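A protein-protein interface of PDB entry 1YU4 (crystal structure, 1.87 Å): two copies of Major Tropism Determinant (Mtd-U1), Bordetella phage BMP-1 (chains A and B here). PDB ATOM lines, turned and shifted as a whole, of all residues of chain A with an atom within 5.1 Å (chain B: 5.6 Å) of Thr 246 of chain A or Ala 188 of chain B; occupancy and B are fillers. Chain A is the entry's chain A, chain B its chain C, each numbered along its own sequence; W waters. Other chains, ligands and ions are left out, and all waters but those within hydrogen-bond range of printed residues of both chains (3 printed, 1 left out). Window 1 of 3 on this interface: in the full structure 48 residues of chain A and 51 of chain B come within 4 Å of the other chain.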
ATOM      1  N   PHE A 225      28.699 -20.376  -7.018  1.00  0.00           N
ATOM      2  CA  PHE A 225      28.751 -19.939  -8.411  1.00  0.00           C
ATOM      3  C   PHE A 225      30.195 -19.798  -8.915  1.00  0.00           C
ATOM      4  O   PHE A 225      30.560 -18.793  -9.520  1.00  0.00           O
ATOM      5  CB  PHE A 225      27.963 -18.634  -8.585  1.00  0.00           C
ATOM      6  CG  PHE A 225      26.508 -18.743  -8.183  1.00  0.00           C
ATOM      7  CD1 PHE A 225      25.573 -19.274  -9.052  1.00  0.00           C
ATOM      8  CD2 PHE A 225      26.081 -18.315  -6.940  1.00  0.00           C
ATOM      9  CE1 PHE A 225      24.235 -19.377  -8.689  1.00  0.00           C
ATOM     10  CE2 PHE A 225      24.747 -18.412  -6.571  1.00  0.00           C
ATOM     11  CZ  PHE A 225      23.822 -18.946  -7.452  1.00  0.00           C
ATOM     12  N   ALA A 242      23.651  -9.429  -6.314  1.00  0.00           N
ATOM     13  CA  ALA A 242      22.439 -10.246  -6.325  1.00  0.00           C
ATOM     14  C   ALA A 242      22.788 -11.719  -6.123  1.00  0.00           C
ATOM     15  O   ALA A 242      22.103 -12.444  -5.405  1.00  0.00           O
ATOM     16  CB  ALA A 242      21.683 -10.053  -7.628  1.00  0.00           C
ATOM     17  N   GLU A 243      23.878 -12.147  -6.743  1.00  0.00           N
ATOM     18  CA  GLU A 243      24.346 -13.517  -6.633  1.00  0.00           C
ATOM     19  C   GLU A 243      24.767 -13.860  -5.209  1.00  0.00           C
ATOM     20  O   GLU A 243      24.457 -14.941  -4.701  1.00  0.00           O
ATOM     21  CB  GLU A 243      25.529 -13.717  -7.570  1.00  0.00           C
ATOM     22  CG  GLU A 243      25.986 -15.148  -7.708  1.00  0.00           C
ATOM     23  CD  GLU A 243      26.820 -15.344  -8.960  1.00  0.00           C
ATOM     24  OE1 GLU A 243      28.060 -15.403  -8.838  1.00  0.00           O
ATOM     25  OE2 GLU A 243      26.225 -15.419 -10.061  1.00  0.00           O
ATOM     26  N   VAL A 244      25.477 -12.936  -4.571  1.00  0.00           N
ATOM     27  CA  VAL A 244      25.928 -13.130  -3.200  1.00  0.00           C
ATOM     28  C   VAL A 244      24.717 -13.304  -2.287  1.00  0.00           C
ATOM     29  O   VAL A 244      24.719 -14.155  -1.399  1.00  0.00           O
ATOM     30  CB  VAL A 244      26.817 -11.955  -2.709  1.00  0.00           C
ATOM     31  CG1 VAL A 244      26.999 -12.004  -1.200  1.00  0.00           C
ATOM     32  CG2 VAL A 244      28.176 -11.989  -3.398  1.00  0.00           C
ATOM     33  N   MET A 245      23.676 -12.510  -2.504  1.00  0.00           N
ATOM     34  CA  MET A 245      22.468 -12.640  -1.685  1.00  0.00           C
ATOM     35  C   MET A 245      21.817 -14.003  -1.901  1.00  0.00           C
ATOM     36  O   MET A 245      21.395 -14.640  -0.939  1.00  0.00           O
ATOM     37  CB  MET A 245      21.478 -11.514  -1.977  1.00  0.00           C
ATOM     38  CG  MET A 245      21.935 -10.153  -1.474  1.00  0.00           C
ATOM     39  SD  MET A 245      22.554 -10.194   0.220  1.00  0.00           S
ATOM     40  CE  MET A 245      23.270  -8.564   0.352  1.00  0.00           C
ATOM     41  N   THR A 246      21.757 -14.455  -3.148  1.00  0.00           N
ATOM     42  CA  THR A 246      21.169 -15.761  -3.465  1.00  0.00           C
ATOM     43  C   THR A 246      21.918 -16.884  -2.736  1.00  0.00           C
ATOM     44  O   THR A 246      21.294 -17.765  -2.163  1.00  0.00           O
ATOM     45  CB  THR A 246      21.180 -16.006  -4.979  1.00  0.00           C
ATOM     46  OG1 THR A 246      20.340 -15.048  -5.629  1.00  0.00           O
ATOM     47  CG2 THR A 246      20.557 -17.350  -5.330  1.00  0.00           C
ATOM     48  N   HIS A 247      23.249 -16.824  -2.764  1.00  0.00           N
ATOM     49  CA  HIS A 247      24.127 -17.741  -2.024  1.00  0.00           C
ATOM     50  C   HIS A 247      23.672 -17.920  -0.578  1.00  0.00           C
ATOM     51  O   HIS A 247      23.602 -19.040  -0.076  1.00  0.00           O
ATOM     52  CB  HIS A 247      25.567 -17.201  -2.030  1.00  0.00           C
ATOM     53  CG  HIS A 247      26.561 -18.060  -1.301  1.00  0.00           C
ATOM     54  ND1 HIS A 247      26.255 -18.750  -0.148  1.00  0.00           N
ATOM     55  CD2 HIS A 247      27.865 -18.321  -1.552  1.00  0.00           C
ATOM     56  CE1 HIS A 247      27.321 -19.408   0.271  1.00  0.00           C
ATOM     57  NE2 HIS A 247      28.312 -19.165  -0.566  1.00  0.00           N
ATOM     58  N   HIS A 248      23.373 -16.804   0.078  1.00  0.00           N
ATOM     59  CA  HIS A 248      23.003 -16.799   1.498  1.00  0.00           C
ATOM     60  C   HIS A 248      21.496 -16.912   1.776  1.00  0.00           C
ATOM     61  O   HIS A 248      21.057 -16.716   2.914  1.00  0.00           O
ATOM     62  CB  HIS A 248      23.567 -15.538   2.151  1.00  0.00           C
ATOM     63  CG  HIS A 248      25.059 -15.539   2.260  1.00  0.00           C
ATOM     64  ND1 HIS A 248      25.872 -14.907   1.345  1.00  0.00           N
ATOM     65  CD2 HIS A 248      25.887 -16.111   3.167  1.00  0.00           C
ATOM     66  CE1 HIS A 248      27.137 -15.076   1.693  1.00  0.00           C
ATOM     67  NE2 HIS A 248      27.174 -15.806   2.794  1.00  0.00           N
ATOM     68  N   GLY A 249      20.709 -17.223   0.749  1.00  0.00           N
ATOM     69  CA  GLY A 249      19.274 -17.409   0.903  1.00  0.00           C
ATOM     70  C   GLY A 249      18.528 -16.103   1.100  1.00  0.00           C
ATOM     71  O   GLY A 249      17.496 -16.060   1.773  1.00  0.00           O
ATOM     72  N   LYS A 250      19.055 -15.045   0.495  1.00  0.00           N
ATOM     73  CA  LYS A 250      18.529 -13.697   0.643  1.00  0.00           C
ATOM     74  C   LYS A 250      18.322 -13.054  -0.725  1.00  0.00           C
ATOM     75  O   LYS A 250      18.547 -13.669  -1.773  1.00  0.00           O
ATOM     76  CB  LYS A 250      19.482 -12.852   1.499  1.00  0.00           C
ATOM     77  CG  LYS A 250      19.550 -13.292   2.963  1.00  0.00           C
ATOM     78  CD  LYS A 250      20.722 -12.673   3.702  1.00  0.00           C
ATOM     79  CE  LYS A 250      20.944 -13.354   5.050  1.00  0.00           C
ATOM     80  NZ  LYS A 250      21.719 -12.509   5.997  1.00  0.00           N
ATOM     81  N   LEU B 184      16.774 -27.580  -6.981  1.00  0.00           N
ATOM     82  CA  LEU B 184      17.087 -26.549  -6.003  1.00  0.00           C
ATOM     83  C   LEU B 184      18.334 -25.791  -6.436  1.00  0.00           C
ATOM     84  O   LEU B 184      19.418 -26.365  -6.527  1.00  0.00           O
ATOM     85  CB  LEU B 184      17.296 -27.171  -4.617  1.00  0.00           C
ATOM     86  CG  LEU B 184      17.563 -26.211  -3.447  1.00  0.00           C
ATOM     87  CD1 LEU B 184      16.483 -25.130  -3.335  1.00  0.00           C
ATOM     88  CD2 LEU B 184      17.664 -26.998  -2.139  1.00  0.00           C
ATOM     89  N   VAL B 185      18.163 -24.498  -6.700  1.00  0.00           N
ATOM     90  CA  VAL B 185      19.229 -23.629  -7.178  1.00  0.00           C
ATOM     91  C   VAL B 185      19.925 -22.941  -6.016  1.00  0.00           C
ATOM     92  O   VAL B 185      19.339 -22.082  -5.361  1.00  0.00           O
ATOM     93  CB  VAL B 185      18.673 -22.547  -8.132  1.00  0.00           C
ATOM     94  CG1 VAL B 185      19.783 -21.597  -8.563  1.00  0.00           C
ATOM     95  CG2 VAL B 185      18.002 -23.201  -9.333  1.00  0.00           C
ATOM     96  N   ALA B 186      21.175 -23.327  -5.770  1.00  0.00           N
ATOM     97  CA  ALA B 186      22.017 -22.718  -4.747  1.00  0.00           C
ATOM     98  C   ALA B 186      21.380 -22.693  -3.346  1.00  0.00           C
ATOM     99  O   ALA B 186      21.691 -21.821  -2.528  1.00  0.00           O
ATOM    100  CB  ALA B 186      22.405 -21.308  -5.184  1.00  0.00           C
ATOM    101  N   GLY B 187      20.475 -23.637  -3.081  1.00  0.00           N
ATOM    102  CA  GLY B 187      19.791 -23.714  -1.799  1.00  0.00           C
ATOM    103  C   GLY B 187      18.729 -22.645  -1.557  1.00  0.00           C
ATOM    104  O   GLY B 187      18.116 -22.635  -0.493  1.00  0.00           O
ATOM    105  N   ALA B 188      18.473 -21.792  -2.552  1.00  0.00           N
ATOM    106  CA  ALA B 188      17.665 -20.577  -2.382  1.00  0.00           C
ATOM    107  C   ALA B 188      16.223 -20.706  -2.882  1.00  0.00           C
ATOM    108  O   ALA B 188      15.302 -20.170  -2.267  1.00  0.00           O
ATOM    109  CB  ALA B 188      18.348 -19.404  -3.081  1.00  0.00           C
ATOM    110  N   PHE B 189      16.039 -21.389  -4.010  1.00  0.00           N
ATOM    111  CA  PHE B 189      14.726 -21.535  -4.648  1.00  0.00           C
ATOM    112  C   PHE B 189      14.753 -22.680  -5.661  1.00  0.00           C
ATOM    113  O   PHE B 189      15.824 -23.141  -6.042  1.00  0.00           O
ATOM    114  CB  PHE B 189      14.326 -20.235  -5.364  1.00  0.00           C
ATOM    115  CG  PHE B 189      15.182 -19.918  -6.559  1.00  0.00           C
ATOM    116  CD1 PHE B 189      14.819 -20.356  -7.828  1.00  0.00           C
ATOM    117  CD2 PHE B 189      16.364 -19.202  -6.410  1.00  0.00           C
ATOM    118  CE1 PHE B 189      15.621 -20.082  -8.931  1.00  0.00           C
ATOM    119  CE2 PHE B 189      17.165 -18.918  -7.508  1.00  0.00           C
ATOM    120  CZ  PHE B 189      16.796 -19.364  -8.767  1.00  0.00           C
ATOM    121  N   TRP B 190      13.580 -23.117  -6.114  1.00  0.00           N
ATOM    122  CA  TRP B 190      13.502 -24.193  -7.102  1.00  0.00           C
ATOM    123  C   TRP B 190      13.183 -23.672  -8.492  1.00  0.00           C
ATOM    124  O   TRP B 190      12.435 -22.713  -8.643  1.00  0.00           O
ATOM    125  CB  TRP B 190      12.452 -25.230  -6.701  1.00  0.00           C
ATOM    126  CG  TRP B 190      12.757 -25.867  -5.410  1.00  0.00           C
ATOM    127  CD1 TRP B 190      12.589 -25.314  -4.186  1.00  0.00           C
ATOM    128  CD2 TRP B 190      13.294 -27.177  -5.192  1.00  0.00           C
ATOM    129  NE1 TRP B 190      12.983 -26.194  -3.212  1.00  0.00           N
ATOM    130  CE2 TRP B 190      13.422 -27.349  -3.801  1.00  0.00           C
ATOM    131  CE3 TRP B 190      13.669 -28.235  -6.032  1.00  0.00           C
ATOM    132  CZ2 TRP B 190      13.915 -28.522  -3.230  1.00  0.00           C
ATOM    133  CZ3 TRP B 190      14.157 -29.397  -5.465  1.00  0.00           C
ATOM    134  CH2 TRP B 190      14.281 -29.530  -4.080  1.00  0.00           C
ATOM    135  N   ASN B 256      17.430 -11.973 -10.888  1.00  0.00           N
ATOM    136  CA  ASN B 256      18.263 -12.586  -9.859  1.00  0.00           C
ATOM    137  C   ASN B 256      18.143 -14.111  -9.909  1.00  0.00           C
ATOM    138  O   ASN B 256      19.148 -14.818  -9.857  1.00  0.00           O
ATOM    139  CB  ASN B 256      17.957 -12.019  -8.460  1.00  0.00           C
ATOM    140  CG  ASN B 256      16.575 -12.395  -7.936  1.00  0.00           C
ATOM    141  OD1 ASN B 256      15.588 -12.391  -8.674  1.00  0.00           O
ATOM    142  ND2 ASN B 256      16.497 -12.689  -6.640  1.00  0.00           N
ATOM    143  N   ALA B 260      21.012 -17.150 -11.523  1.00  0.00           N
ATOM    144  CA  ALA B 260      21.374 -18.224 -10.605  1.00  0.00           C
ATOM    145  C   ALA B 260      21.073 -19.593 -11.209  1.00  0.00           C
ATOM    146  O   ALA B 260      21.937 -20.475 -11.225  1.00  0.00           O
ATOM    147  CB  ALA B 260      20.655 -18.051  -9.285  1.00  0.00           C
ATOM    148  N   ASP B 376       9.283 -20.889  -4.531  1.00  0.00           N
ATOM    149  CA  ASP B 376      10.018 -20.791  -3.275  1.00  0.00           C
ATOM    150  C   ASP B 376      10.451 -22.160  -2.771  1.00  0.00           C
ATOM    151  O   ASP B 376       9.833 -23.179  -3.088  1.00  0.00           O
ATOM    152  CB  ASP B 376       9.161 -20.128  -2.187  1.00  0.00           C
ATOM    153  CG  ASP B 376       9.020 -18.633  -2.377  1.00  0.00           C
ATOM    154  OD1 ASP B 376       9.385 -18.117  -3.451  1.00  0.00           O
ATOM    155  OD2 ASP B 376       8.554 -17.887  -1.489  1.00  0.00           O
ATOM    156  N   HIS B 377      11.524 -22.161  -1.987  1.00  0.00           N
ATOM    157  CA  HIS B 377      11.973 -23.329  -1.257  1.00  0.00           C
ATOM    158  C   HIS B 377      11.232 -23.367   0.079  1.00  0.00           C
ATOM    159  O   HIS B 377      11.188 -22.375   0.808  1.00  0.00           O
ATOM    160  CB  HIS B 377      13.483 -23.256  -1.027  1.00  0.00           C
ATOM    161  CG  HIS B 377      14.024 -24.365  -0.179  1.00  0.00           C
ATOM    162  ND1 HIS B 377      14.830 -24.131   0.913  1.00  0.00           N
ATOM    163  CD2 HIS B 377      13.885 -25.708  -0.264  1.00  0.00           C
ATOM    164  CE1 HIS B 377      15.155 -25.284   1.469  1.00  0.00           C
ATOM    165  NE2 HIS B 377      14.600 -26.256   0.770  1.00  0.00           N
HETATM  166  O   HOH W   1      16.246 -18.273  -0.425  1.00  0.00           O
HETATM  167  O   HOH W   2      21.251 -14.051  -8.270  1.00  0.00           O
HETATM  168  O   HOH W   3      19.510 -12.031  -5.222  1.00  0.00           O
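Of the printed residues of chain B, Thr 246 of chain A touches Ala 188 (3.5 Å). Printed residues of chain A within 4 Å of Ala 188 of chain B: Thr 246. Of the printed residues of chain A, Ala 186 of chain B touches Phe 225. Of the printed residues of chain A, Ala 260 of chain B touches Phe 225. Of the printed residues of chain B, Phe 225 of chain A touches Ala 186 (3.6 Å) and Ala 260 (3.6 Å). Met 245 of chain A touches none of the printed residues of chain B. Ala 242 of chain A touches none of the printed residues of chain B. The nearest printed residue of chain B that does not touch Thr 246 of chain A is Ala 260 of chain B (4.02 Å). The nearest printed residue of chain B that does not touch Phe 225 of chain A is Val 185 of chain B (5.0 Å).
Printed residues of chain B that touch a printed residue of chain A: Ala 186, Ala 188 and Ala 260. Along chain B the printed residues that touch a printed residue of chain A span positions 186 to 260. Of the 10 printed residues of chain A, 2 touch a printed residue of chain B. Along chain A the printed residues that touch a printed residue of chain B span positions 225 to 246. Among the printed residues, 3 pairs touch across the chains. Among the printed residues, no Asp or Glu carboxylate lies within 4 Å of a Lys or Arg side-chain nitrogen of the other chain.
The backbone carbonyl oxygen (O) of Ala 242 of chain A sits at hydrogen-bond distance from the side-chain hydroxyl (OG1) of Thr 246 of chain A, 3.2 Å away.
Ala 186 of chain B touches Phe 225 of chain A (CB to CZ, 3.6 Å). O of Ala 260 of chain B touches CE1 of Phe 225 of chain A (3.6 Å). Ala 188 of chain B touches Thr 246 of chain A (CB to O, 3.5 Å).
No position is printed for both chains.
Water W3 lies within hydrogen-bond range of O of Ala 242 of chain A (2.6 Å), OG1 of Thr 246 of chain A (3.2 Å) and ND2 of Asn 256 of chain B (3.4 Å). Water W2 lies within hydrogen-bond range of O of Asn 256 of chain B (2.7 Å), OG1 of Thr 246 of chain A (3.0 Å) and O of Ala 242 of chain A (3.4 Å). Water W1 lies within hydrogen-bond range of the backbone carbonyl oxygen (O) of Ala 188 of chain B and the backbone carbonyl oxygen (O) of Gly 249 of chain A.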
